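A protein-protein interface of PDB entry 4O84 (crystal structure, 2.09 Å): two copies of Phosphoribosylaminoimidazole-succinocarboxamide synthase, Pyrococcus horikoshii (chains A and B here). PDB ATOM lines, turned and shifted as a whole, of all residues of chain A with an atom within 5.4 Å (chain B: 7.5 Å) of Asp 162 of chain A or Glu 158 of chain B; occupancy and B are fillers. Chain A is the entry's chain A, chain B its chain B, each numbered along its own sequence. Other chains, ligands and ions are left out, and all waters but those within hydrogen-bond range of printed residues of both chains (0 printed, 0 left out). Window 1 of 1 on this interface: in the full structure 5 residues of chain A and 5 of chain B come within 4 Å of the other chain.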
ATOM      1  N   ASN A 157      17.370  13.131 -26.457  1.00  0.00           N
ATOM      2  CA  ASN A 157      16.083  12.456 -26.333  1.00  0.00           C
ATOM      3  C   ASN A 157      14.932  13.345 -26.778  1.00  0.00           C
ATOM      4  O   ASN A 157      14.084  12.913 -27.563  1.00  0.00           O
ATOM      5  CB  ASN A 157      15.818  11.966 -24.907  1.00  0.00           C
ATOM      6  CG  ASN A 157      14.481  11.245 -24.787  1.00  0.00           C
ATOM      7  OD1 ASN A 157      14.247  10.261 -25.494  1.00  0.00           O
ATOM      8  ND2 ASN A 157      13.599  11.724 -23.886  1.00  0.00           N
ATOM      9  N   GLU A 158      14.906  14.579 -26.282  1.00  0.00           N
ATOM     10  CA  GLU A 158      13.778  15.453 -26.552  1.00  0.00           C
ATOM     11  C   GLU A 158      13.675  15.777 -28.052  1.00  0.00           C
ATOM     12  O   GLU A 158      12.586  15.757 -28.618  1.00  0.00           O
ATOM     13  CB  GLU A 158      13.819  16.733 -25.705  1.00  0.00           C
ATOM     14  CG  GLU A 158      12.430  17.303 -25.392  1.00  0.00           C
ATOM     15  CD  GLU A 158      11.524  16.315 -24.663  1.00  0.00           C
ATOM     16  OE1 GLU A 158      12.026  15.487 -23.843  1.00  0.00           O
ATOM     17  OE2 GLU A 158      10.302  16.340 -24.911  1.00  0.00           O
ATOM     18  N   ILE A 159      14.809  16.062 -28.683  1.00  0.00           N
ATOM     19  CA  ILE A 159      14.815  16.404 -30.111  1.00  0.00           C
ATOM     20  C   ILE A 159      14.327  15.224 -30.958  1.00  0.00           C
ATOM     21  O   ILE A 159      13.444  15.370 -31.790  1.00  0.00           O
ATOM     22  CB  ILE A 159      16.209  16.869 -30.566  1.00  0.00           C
ATOM     23  CG1 ILE A 159      16.638  18.102 -29.754  1.00  0.00           C
ATOM     24  CG2 ILE A 159      16.209  17.187 -32.062  1.00  0.00           C
ATOM     25  CD1 ILE A 159      18.134  18.345 -29.754  1.00  0.00           C
ATOM     26  N   LEU A 160      14.874  14.046 -30.707  1.00  0.00           N
ATOM     27  CA  LEU A 160      14.490  12.871 -31.484  1.00  0.00           C
ATOM     28  C   LEU A 160      13.027  12.496 -31.242  1.00  0.00           C
ATOM     29  O   LEU A 160      12.281  12.264 -32.209  1.00  0.00           O
ATOM     30  CB  LEU A 160      15.441  11.694 -31.237  1.00  0.00           C
ATOM     31  CG  LEU A 160      16.920  11.885 -31.653  1.00  0.00           C
ATOM     32  CD1 LEU A 160      17.708  10.629 -31.377  1.00  0.00           C
ATOM     33  CD2 LEU A 160      17.122  12.288 -33.105  1.00  0.00           C
ATOM     34  N   LYS A 161      12.608  12.504 -29.972  1.00  0.00           N
ATOM     35  CA  LYS A 161      11.238  12.150 -29.604  1.00  0.00           C
ATOM     36  C   LYS A 161      10.208  13.046 -30.302  1.00  0.00           C
ATOM     37  O   LYS A 161       9.228  12.545 -30.875  1.00  0.00           O
ATOM     38  CB  LYS A 161      11.018  12.224 -28.081  1.00  0.00           C
ATOM     39  CG  LYS A 161       9.617  11.799 -27.647  1.00  0.00           C
ATOM     40  CD  LYS A 161       9.352  12.025 -26.157  1.00  0.00           C
ATOM     41  CE  LYS A 161       9.536  13.491 -25.791  1.00  0.00           C
ATOM     42  NZ  LYS A 161       8.972  13.872 -24.474  1.00  0.00           N
ATOM     43  N   ASP A 162      10.439  14.361 -30.245  1.00  0.00           N
ATOM     44  CA  ASP A 162       9.508  15.316 -30.820  1.00  0.00           C
ATOM     45  C   ASP A 162       9.497  15.250 -32.347  1.00  0.00           C
ATOM     46  O   ASP A 162       8.447  15.246 -32.973  1.00  0.00           O
ATOM     47  CB  ASP A 162       9.829  16.717 -30.327  1.00  0.00           C
ATOM     48  CG  ASP A 162       9.713  16.836 -28.825  1.00  0.00           C
ATOM     49  OD1 ASP A 162       9.162  15.906 -28.168  1.00  0.00           O
ATOM     50  OD2 ASP A 162      10.206  17.850 -28.299  1.00  0.00           O
ATOM     51  N   TYR A 163      10.679  15.178 -32.939  1.00  0.00           N
ATOM     52  CA  TYR A 163      10.808  14.994 -34.381  1.00  0.00           C
ATOM     53  C   TYR A 163      10.012  13.766 -34.863  1.00  0.00           C
ATOM     54  O   TYR A 163       9.212  13.844 -35.808  1.00  0.00           O
ATOM     55  CB  TYR A 163      12.289  14.849 -34.722  1.00  0.00           C
ATOM     56  CG  TYR A 163      12.590  14.702 -36.194  1.00  0.00           C
ATOM     57  CD1 TYR A 163      12.545  15.800 -37.050  1.00  0.00           C
ATOM     58  CD2 TYR A 163      12.951  13.472 -36.712  1.00  0.00           C
ATOM     59  CE1 TYR A 163      12.840  15.665 -38.404  1.00  0.00           C
ATOM     60  CE2 TYR A 163      13.234  13.313 -38.060  1.00  0.00           C
ATOM     61  CZ  TYR A 163      13.181  14.412 -38.904  1.00  0.00           C
ATOM     62  OH  TYR A 163      13.470  14.242 -40.239  1.00  0.00           O
ATOM     63  N   LEU A 164      10.211  12.648 -34.173  1.00  0.00           N
ATOM     64  CA  LEU A 164       9.565  11.392 -34.550  1.00  0.00           C
ATOM     65  C   LEU A 164       8.076  11.366 -34.286  1.00  0.00           C
ATOM     66  O   LEU A 164       7.319  10.790 -35.088  1.00  0.00           O
ATOM     67  CB  LEU A 164      10.260  10.187 -33.912  1.00  0.00           C
ATOM     68  CG  LEU A 164      11.707   9.973 -34.381  1.00  0.00           C
ATOM     69  CD1 LEU A 164      12.394   8.921 -33.514  1.00  0.00           C
ATOM     70  CD2 LEU A 164      11.773   9.586 -35.859  1.00  0.00           C
ATOM     71  N   ALA A 165       7.659  11.999 -33.185  1.00  0.00           N
ATOM     72  CA  ALA A 165       6.243  12.075 -32.791  1.00  0.00           C
ATOM     73  C   ALA A 165       5.392  12.745 -33.868  1.00  0.00           C
ATOM     74  O   ALA A 165       4.254  12.339 -34.102  1.00  0.00           O
ATOM     75  CB  ALA A 165       6.077  12.821 -31.461  1.00  0.00           C
ATOM     76  N   LYS A 166       5.951  13.773 -34.519  1.00  0.00           N
ATOM     77  CA  LYS A 166       5.249  14.481 -35.594  1.00  0.00           C
ATOM     78  C   LYS A 166       5.027  13.578 -36.800  1.00  0.00           C
ATOM     79  O   LYS A 166       4.172  13.858 -37.634  1.00  0.00           O
ATOM     80  CB  LYS A 166       6.006  15.747 -36.016  1.00  0.00           C
ATOM     81  CG  LYS A 166       6.084  16.774 -34.901  1.00  0.00           C
ATOM     82  CD  LYS A 166       7.063  17.898 -35.200  1.00  0.00           C
ATOM     83  CE  LYS A 166       7.204  18.761 -33.954  1.00  0.00           C
ATOM     84  NZ  LYS A 166       8.349  19.705 -34.042  1.00  0.00           N
ATOM     85  N   LEU B  60      -2.769  19.527 -18.205  1.00  0.00           N
ATOM     86  CA  LEU B  60      -1.626  19.915 -17.363  1.00  0.00           C
ATOM     87  C   LEU B  60      -1.691  19.282 -15.979  1.00  0.00           C
ATOM     88  O   LEU B  60      -0.672  18.808 -15.440  1.00  0.00           O
ATOM     89  CB  LEU B  60      -1.525  21.449 -17.273  1.00  0.00           C
ATOM     90  CG  LEU B  60      -1.127  22.104 -18.603  1.00  0.00           C
ATOM     91  CD1 LEU B  60      -1.213  23.620 -18.516  1.00  0.00           C
ATOM     92  CD2 LEU B  60       0.255  21.666 -19.071  1.00  0.00           C
ATOM     93  N   VAL B  92       6.650  32.060 -22.692  1.00  0.00           N
ATOM     94  CA  VAL B  92       7.541  31.018 -23.208  1.00  0.00           C
ATOM     95  C   VAL B  92       7.491  30.993 -24.720  1.00  0.00           C
ATOM     96  O   VAL B  92       6.407  31.029 -25.299  1.00  0.00           O
ATOM     97  CB  VAL B  92       7.237  29.626 -22.617  1.00  0.00           C
ATOM     98  CG1 VAL B  92       8.300  28.617 -23.047  1.00  0.00           C
ATOM     99  CG2 VAL B  92       7.200  29.709 -21.109  1.00  0.00           C
ATOM    100  N   ASN B  94       9.081  29.294 -28.380  1.00  0.00           N
ATOM    101  CA  ASN B  94       9.752  28.202 -29.083  1.00  0.00           C
ATOM    102  C   ASN B  94      10.199  28.607 -30.475  1.00  0.00           C
ATOM    103  O   ASN B  94      11.169  28.080 -31.007  1.00  0.00           O
ATOM    104  CB  ASN B  94       8.816  26.996 -29.205  1.00  0.00           C
ATOM    105  CG  ASN B  94       8.378  26.454 -27.853  1.00  0.00           C
ATOM    106  OD1 ASN B  94       9.202  26.104 -27.013  1.00  0.00           O
ATOM    107  ND2 ASN B  94       7.069  26.394 -27.640  1.00  0.00           N
ATOM    108  N   PRO B 115      13.778  26.599 -25.546  1.00  0.00           N
ATOM    109  CA  PRO B 115      12.711  27.565 -25.271  1.00  0.00           C
ATOM    110  C   PRO B 115      13.243  28.758 -24.484  1.00  0.00           C
ATOM    111  O   PRO B 115      14.113  28.602 -23.638  1.00  0.00           O
ATOM    112  CB  PRO B 115      11.704  26.775 -24.426  1.00  0.00           C
ATOM    113  CG  PRO B 115      12.111  25.345 -24.523  1.00  0.00           C
ATOM    114  CD  PRO B 115      13.570  25.316 -24.857  1.00  0.00           C
ATOM    115  N   ILE B 152       8.162  25.646 -13.742  1.00  0.00           N
ATOM    116  CA  ILE B 152       6.794  25.274 -14.108  1.00  0.00           C
ATOM    117  C   ILE B 152       6.486  25.684 -15.542  1.00  0.00           C
ATOM    118  O   ILE B 152       5.967  24.888 -16.324  1.00  0.00           O
ATOM    119  CB  ILE B 152       5.733  25.836 -13.122  1.00  0.00           C
ATOM    120  CG1 ILE B 152       6.023  25.331 -11.704  1.00  0.00           C
ATOM    121  CG2 ILE B 152       4.353  25.346 -13.494  1.00  0.00           C
ATOM    122  CD1 ILE B 152       5.267  26.064 -10.609  1.00  0.00           C
ATOM    123  N   ALA B 153       6.817  26.922 -15.895  1.00  0.00           N
ATOM    124  CA  ALA B 153       6.546  27.413 -17.251  1.00  0.00           C
ATOM    125  C   ALA B 153       7.150  26.505 -18.346  1.00  0.00           C
ATOM    126  O   ALA B 153       6.495  26.222 -19.359  1.00  0.00           O
ATOM    127  CB  ALA B 153       7.010  28.843 -17.407  1.00  0.00           C
ATOM    128  N   LEU B 154       8.381  26.033 -18.125  1.00  0.00           N
ATOM    129  CA  LEU B 154       9.056  25.211 -19.113  1.00  0.00           C
ATOM    130  C   LEU B 154       8.453  23.802 -19.217  1.00  0.00           C
ATOM    131  O   LEU B 154       8.396  23.223 -20.314  1.00  0.00           O
ATOM    132  CB  LEU B 154      10.564  25.158 -18.855  1.00  0.00           C
ATOM    133  CG  LEU B 154      11.264  26.478 -19.211  1.00  0.00           C
ATOM    134  CD1 LEU B 154      12.622  26.594 -18.528  1.00  0.00           C
ATOM    135  CD2 LEU B 154      11.388  26.639 -20.724  1.00  0.00           C
ATOM    136  N   LYS B 155       8.004  23.278 -18.078  1.00  0.00           N
ATOM    137  CA  LYS B 155       7.290  22.024 -18.014  1.00  0.00           C
ATOM    138  C   LYS B 155       5.953  22.137 -18.784  1.00  0.00           C
ATOM    139  O   LYS B 155       5.648  21.322 -19.659  1.00  0.00           O
ATOM    140  CB  LYS B 155       7.059  21.688 -16.550  1.00  0.00           C
ATOM    141  CG  LYS B 155       6.789  20.221 -16.264  1.00  0.00           C
ATOM    142  CD  LYS B 155       7.113  19.923 -14.803  1.00  0.00           C
ATOM    143  N   VAL B 156       5.182  23.178 -18.471  1.00  0.00           N
ATOM    144  CA  VAL B 156       3.953  23.461 -19.183  1.00  0.00           C
ATOM    145  C   VAL B 156       4.227  23.594 -20.689  1.00  0.00           C
ATOM    146  O   VAL B 156       3.494  23.033 -21.499  1.00  0.00           O
ATOM    147  CB  VAL B 156       3.249  24.728 -18.634  1.00  0.00           C
ATOM    148  CG1 VAL B 156       2.104  25.167 -19.562  1.00  0.00           C
ATOM    149  CG2 VAL B 156       2.738  24.477 -17.217  1.00  0.00           C
ATOM    150  N   ASN B 157       5.269  24.350 -21.048  1.00  0.00           N
ATOM    151  CA  ASN B 157       5.652  24.492 -22.439  1.00  0.00           C
ATOM    152  C   ASN B 157       5.827  23.139 -23.123  1.00  0.00           C
ATOM    153  O   ASN B 157       5.283  22.926 -24.197  1.00  0.00           O
ATOM    154  CB  ASN B 157       6.935  25.292 -22.594  1.00  0.00           C
ATOM    155  CG  ASN B 157       7.345  25.452 -24.048  1.00  0.00           C
ATOM    156  OD1 ASN B 157       6.582  25.986 -24.867  1.00  0.00           O
ATOM    157  ND2 ASN B 157       8.569  24.996 -24.381  1.00  0.00           N
ATOM    158  N   GLU B 158       6.573  22.234 -22.484  1.00  0.00           N
ATOM    159  CA  GLU B 158       6.880  20.953 -23.113  1.00  0.00           C
ATOM    160  C   GLU B 158       5.640  20.084 -23.341  1.00  0.00           C
ATOM    161  O   GLU B 158       5.480  19.500 -24.418  1.00  0.00           O
ATOM    162  CB  GLU B 158       7.974  20.177 -22.358  1.00  0.00           C
ATOM    163  CG  GLU B 158       8.796  19.307 -23.317  1.00  0.00           C
ATOM    164  CD  GLU B 158       9.557  20.116 -24.383  1.00  0.00           C
ATOM    165  OE1 GLU B 158       9.972  21.289 -24.137  1.00  0.00           O
ATOM    166  OE2 GLU B 158       9.759  19.586 -25.485  1.00  0.00           O
ATOM    167  N   ILE B 159       4.779  20.008 -22.331  1.00  0.00           N
ATOM    168  CA  ILE B 159       3.514  19.293 -22.449  1.00  0.00           C
ATOM    169  C   ILE B 159       2.628  19.861 -23.567  1.00  0.00           C
ATOM    170  O   ILE B 159       2.169  19.116 -24.418  1.00  0.00           O
ATOM    171  CB  ILE B 159       2.751  19.280 -21.100  1.00  0.00           C
ATOM    172  CG1 ILE B 159       3.617  18.596 -20.019  1.00  0.00           C
ATOM    173  CG2 ILE B 159       1.367  18.642 -21.262  1.00  0.00           C
ATOM    174  CD1 ILE B 159       3.231  18.909 -18.588  1.00  0.00           C
ATOM    175  N   LEU B 160       2.371  21.164 -23.549  1.00  0.00           N
ATOM    176  CA  LEU B 160       1.508  21.766 -24.548  1.00  0.00           C
ATOM    177  C   LEU B 160       2.085  21.621 -25.955  1.00  0.00           C
ATOM    178  O   LEU B 160       1.378  21.194 -26.861  1.00  0.00           O
ATOM    179  CB  LEU B 160       1.200  23.226 -24.206  1.00  0.00           C
ATOM    180  CG  LEU B 160       0.393  23.544 -22.919  1.00  0.00           C
ATOM    181  CD1 LEU B 160       0.167  25.035 -22.773  1.00  0.00           C
ATOM    182  CD2 LEU B 160      -0.949  22.813 -22.833  1.00  0.00           C
ATOM    183  N   LYS B 161       3.383  21.913 -26.117  1.00  0.00           N
ATOM    184  CA  LYS B 161       4.055  21.871 -27.420  1.00  0.00           C
ATOM    185  C   LYS B 161       3.973  20.493 -28.065  1.00  0.00           C
ATOM    186  O   LYS B 161       3.679  20.372 -29.272  1.00  0.00           O
ATOM    187  CB  LYS B 161       5.528  22.278 -27.302  1.00  0.00           C
ATOM    188  CG  LYS B 161       6.280  22.210 -28.628  1.00  0.00           C
ATOM    189  CD  LYS B 161       7.771  22.423 -28.460  1.00  0.00           C
ATOM    190  CE  LYS B 161       8.385  21.333 -27.601  1.00  0.00           C
ATOM    191  NZ  LYS B 161       9.867  21.371 -27.607  1.00  0.00           N
ATOM    192  N   ASP B 162       4.242  19.469 -27.252  1.00  0.00           N
ATOM    193  CA  ASP B 162       4.238  18.090 -27.742  1.00  0.00           C
ATOM    194  C   ASP B 162       2.838  17.610 -28.073  1.00  0.00           C
ATOM    195  O   ASP B 162       2.654  16.911 -29.065  1.00  0.00           O
ATOM    196  CB  ASP B 162       4.918  17.136 -26.734  1.00  0.00           C
ATOM    197  CG  ASP B 162       6.392  17.482 -26.494  1.00  0.00           C
ATOM    198  OD1 ASP B 162       7.004  18.251 -27.274  1.00  0.00           O
ATOM    199  OD2 ASP B 162       6.961  16.998 -25.506  1.00  0.00           O
ATOM    200  N   TYR B 163       1.874  17.960 -27.220  1.00  0.00           N
ATOM    201  CA  TYR B 163       0.479  17.622 -27.415  1.00  0.00           C
ATOM    202  C   TYR B 163      -0.033  18.243 -28.716  1.00  0.00           C
ATOM    203  O   TYR B 163      -0.668  17.572 -29.521  1.00  0.00           O
ATOM    204  CB  TYR B 163      -0.342  18.135 -26.228  1.00  0.00           C
ATOM    205  CG  TYR B 163      -1.834  17.891 -26.298  1.00  0.00           C
ATOM    206  CD1 TYR B 163      -2.368  16.624 -26.058  1.00  0.00           C
ATOM    207  CD2 TYR B 163      -2.714  18.931 -26.576  1.00  0.00           C
ATOM    208  CE1 TYR B 163      -3.743  16.398 -26.111  1.00  0.00           C
ATOM    209  CE2 TYR B 163      -4.084  18.719 -26.628  1.00  0.00           C
ATOM    210  CZ  TYR B 163      -4.591  17.452 -26.406  1.00  0.00           C
ATOM    211  OH  TYR B 163      -5.951  17.245 -26.456  1.00  0.00           O
ATOM    212  N   LEU B 164       0.259  19.528 -28.915  1.00  0.00           N
ATOM    213  CA  LEU B 164      -0.204  20.236 -30.105  1.00  0.00           C
ATOM    214  C   LEU B 164       0.485  19.782 -31.381  1.00  0.00           C
ATOM    215  O   LEU B 164      -0.158  19.725 -32.433  1.00  0.00           O
ATOM    216  CB  LEU B 164      -0.095  21.754 -29.933  1.00  0.00           C
ATOM    217  CG  LEU B 164      -1.009  22.315 -28.835  1.00  0.00           C
ATOM    218  CD1 LEU B 164      -0.668  23.758 -28.476  1.00  0.00           C
ATOM    219  CD2 LEU B 164      -2.481  22.160 -29.188  1.00  0.00           C
ATOM    220  N   ALA B 165       1.765  19.408 -31.270  1.00  0.00           N
ATOM    221  CA  ALA B 165       2.571  19.031 -32.417  1.00  0.00           C
ATOM    222  C   ALA B 165       2.007  17.787 -33.084  1.00  0.00           C
ATOM    223  O   ALA B 165       2.051  17.666 -34.313  1.00  0.00           O
ATOM    224  CB  ALA B 165       4.026  18.803 -32.011  1.00  0.00           C
ATOM    225  N   LYS B 166       1.486  16.867 -32.268  1.00  0.00           N
ATOM    226  CA  LYS B 166       0.893  15.620 -32.749  1.00  0.00           C
ATOM    227  C   LYS B 166      -0.391  15.905 -33.528  1.00  0.00           C
ATOM    228  O   LYS B 166      -0.901  15.048 -34.253  1.00  0.00           O
ATOM    229  CB  LYS B 166       0.618  14.663 -31.578  1.00  0.00           C
ATOM    230  CG  LYS B 166       1.873  14.196 -30.873  1.00  0.00           C
ATOM    231  CD  LYS B 166       1.555  13.475 -29.573  1.00  0.00           C
ATOM    232  CE  LYS B 166       2.847  13.139 -28.855  1.00  0.00           C
ATOM    233  NZ  LYS B 166       2.606  12.596 -27.492  1.00  0.00           N
ATOM    234  N   LEU B 171       3.169  25.255 -31.301  1.00  0.00           N
ATOM    235  CA  LEU B 171       3.121  26.191 -30.179  1.00  0.00           C
ATOM    236  C   LEU B 171       4.262  27.182 -30.399  1.00  0.00           C
ATOM    237  O   LEU B 171       5.420  26.868 -30.116  1.00  0.00           O
ATOM    238  CB  LEU B 171       3.288  25.471 -28.829  1.00  0.00           C
ATOM    239  CG  LEU B 171       3.091  26.346 -27.578  1.00  0.00           C
ATOM    240  CD1 LEU B 171       1.771  27.105 -27.611  1.00  0.00           C
ATOM    241  CD2 LEU B 171       3.195  25.516 -26.309  1.00  0.00           C
ATOM    242  N   PHE B 174       3.611  31.622 -25.882  1.00  0.00           N
ATOM    243  CA  PHE B 174       2.413  31.782 -25.082  1.00  0.00           C
ATOM    244  C   PHE B 174       2.682  32.494 -23.765  1.00  0.00           C
ATOM    245  O   PHE B 174       3.821  32.505 -23.265  1.00  0.00           O
ATOM    246  CB  PHE B 174       1.669  30.445 -24.857  1.00  0.00           C
ATOM    247  CG  PHE B 174       2.408  29.454 -24.005  1.00  0.00           C
ATOM    248  CD1 PHE B 174       1.919  29.104 -22.762  1.00  0.00           C
ATOM    249  CD2 PHE B 174       3.549  28.818 -24.468  1.00  0.00           C
ATOM    250  CE1 PHE B 174       2.566  28.147 -21.983  1.00  0.00           C
ATOM    251  CE2 PHE B 174       4.215  27.882 -23.686  1.00  0.00           C
ATOM    252  CZ  PHE B 174       3.726  27.544 -22.440  1.00  0.00           C
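Among the printed residues, pairs that only touch across the chains: Lys 166 of chain A with Ala 165 of chain B (3.7 Å).
Printed residues of chain A that touch a printed residue of chain B: Glu 158, Lys 161, Asp 162 and Lys 166. Along chain A the printed residues that touch a printed residue of chain B span positions 158 to 166. Printed residues of chain B that touch a printed residue of chain A: Glu 158, Lys 161, Asp 162 and Ala 165. Hydrophobic or aromatic side chains of chain B that line the printed part of chain A: Ala 165. Along chain B the printed residues that touch a printed residue of chain A span positions 158 to 165.
Asp 162 of chain A touches just these residues of chain B: Glu 158 (3.3 Å), Lys 161 (3.6 Å) and Asp 162 (3.3 Å). Leu 164 of chain A touches none of the printed residues of chain B. Ile 152 of chain B touches none of the printed residues of chain A. Glu 158 of chain B touches two residues of chain A. Printed residues of chain A within 4 Å of Lys 161 of chain B: Asp 162. Printed residues of chain A within 4 Å of Asp 162 of chain B: Glu 158 (3.5 Å), Lys 161 (3.9 Å) and Asp 162 (3.3 Å). Printed residues of chain A within 4 Å of Ala 165 of chain B: Lys 166. The nearest residue of chain B that does not touch Asp 162 of chain A is Ala 165 of chain B (5.8 Å). The nearest printed residue of chain B that does not touch Glu 158 of chain A is Lys 161 of chain B (5.3 Å).
NZ of Lys 161 of chain A lies within salt-bridge range of OE1 of Glu 158 of chain A, at 3.5 Å. The side-chain amino group (NZ) of Lys 161 of chain B lies within salt-bridge range of the side-chain carboxylate (OE1) of Glu 158 of chain B.
The side-chain carboxylate (OD2) of Asp 162 of chain B sits close to the side-chain amino group (NZ) of Lys 161 of chain A, 3.9 Å away. The side-chain carboxylate (OD2) of Asp 162 of chain A lies close to the side-chain amino group (NZ) of Lys 161 of chain B (3.6 Å). OE2 of Glu 158 of chain B lies close to OE2 of Glu 158 of chain A (3.3 Å). The side-chain carboxylate of Glu 158 of chain A lies close to the side-chain carboxylate of Asp 162 of chain B (3.5 Å). The side-chain carboxylate of Glu 158 of chain B sits close to the side-chain carboxylate of Asp 162 of chain A (3.3 Å). The side-chain carboxylate of Asp 162 of chain A sits close to the side-chain carboxylate of Asp 162 of chain B, at 3.3 Å.
Glu 158 of chain A touches its own counterpart, Glu 158 of chain B. Lys 161 of chain A touches Asp 162 of chain B, and with the chains exchanged Asp 162 of chain A touches Lys 161 of chain B. Asp 162 of chain B touches its own counterpart, Asp 162 of chain A. Lys 166 of chain A touches Ala 165 of chain B, but with the chains exchanged Ala 165 of chain A does not touch Lys 166 of chain B (4.2 Å). Of the 7 pairs that touch across the chains among the printed residues, 6 have their exchanged pair printed and touching as well.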
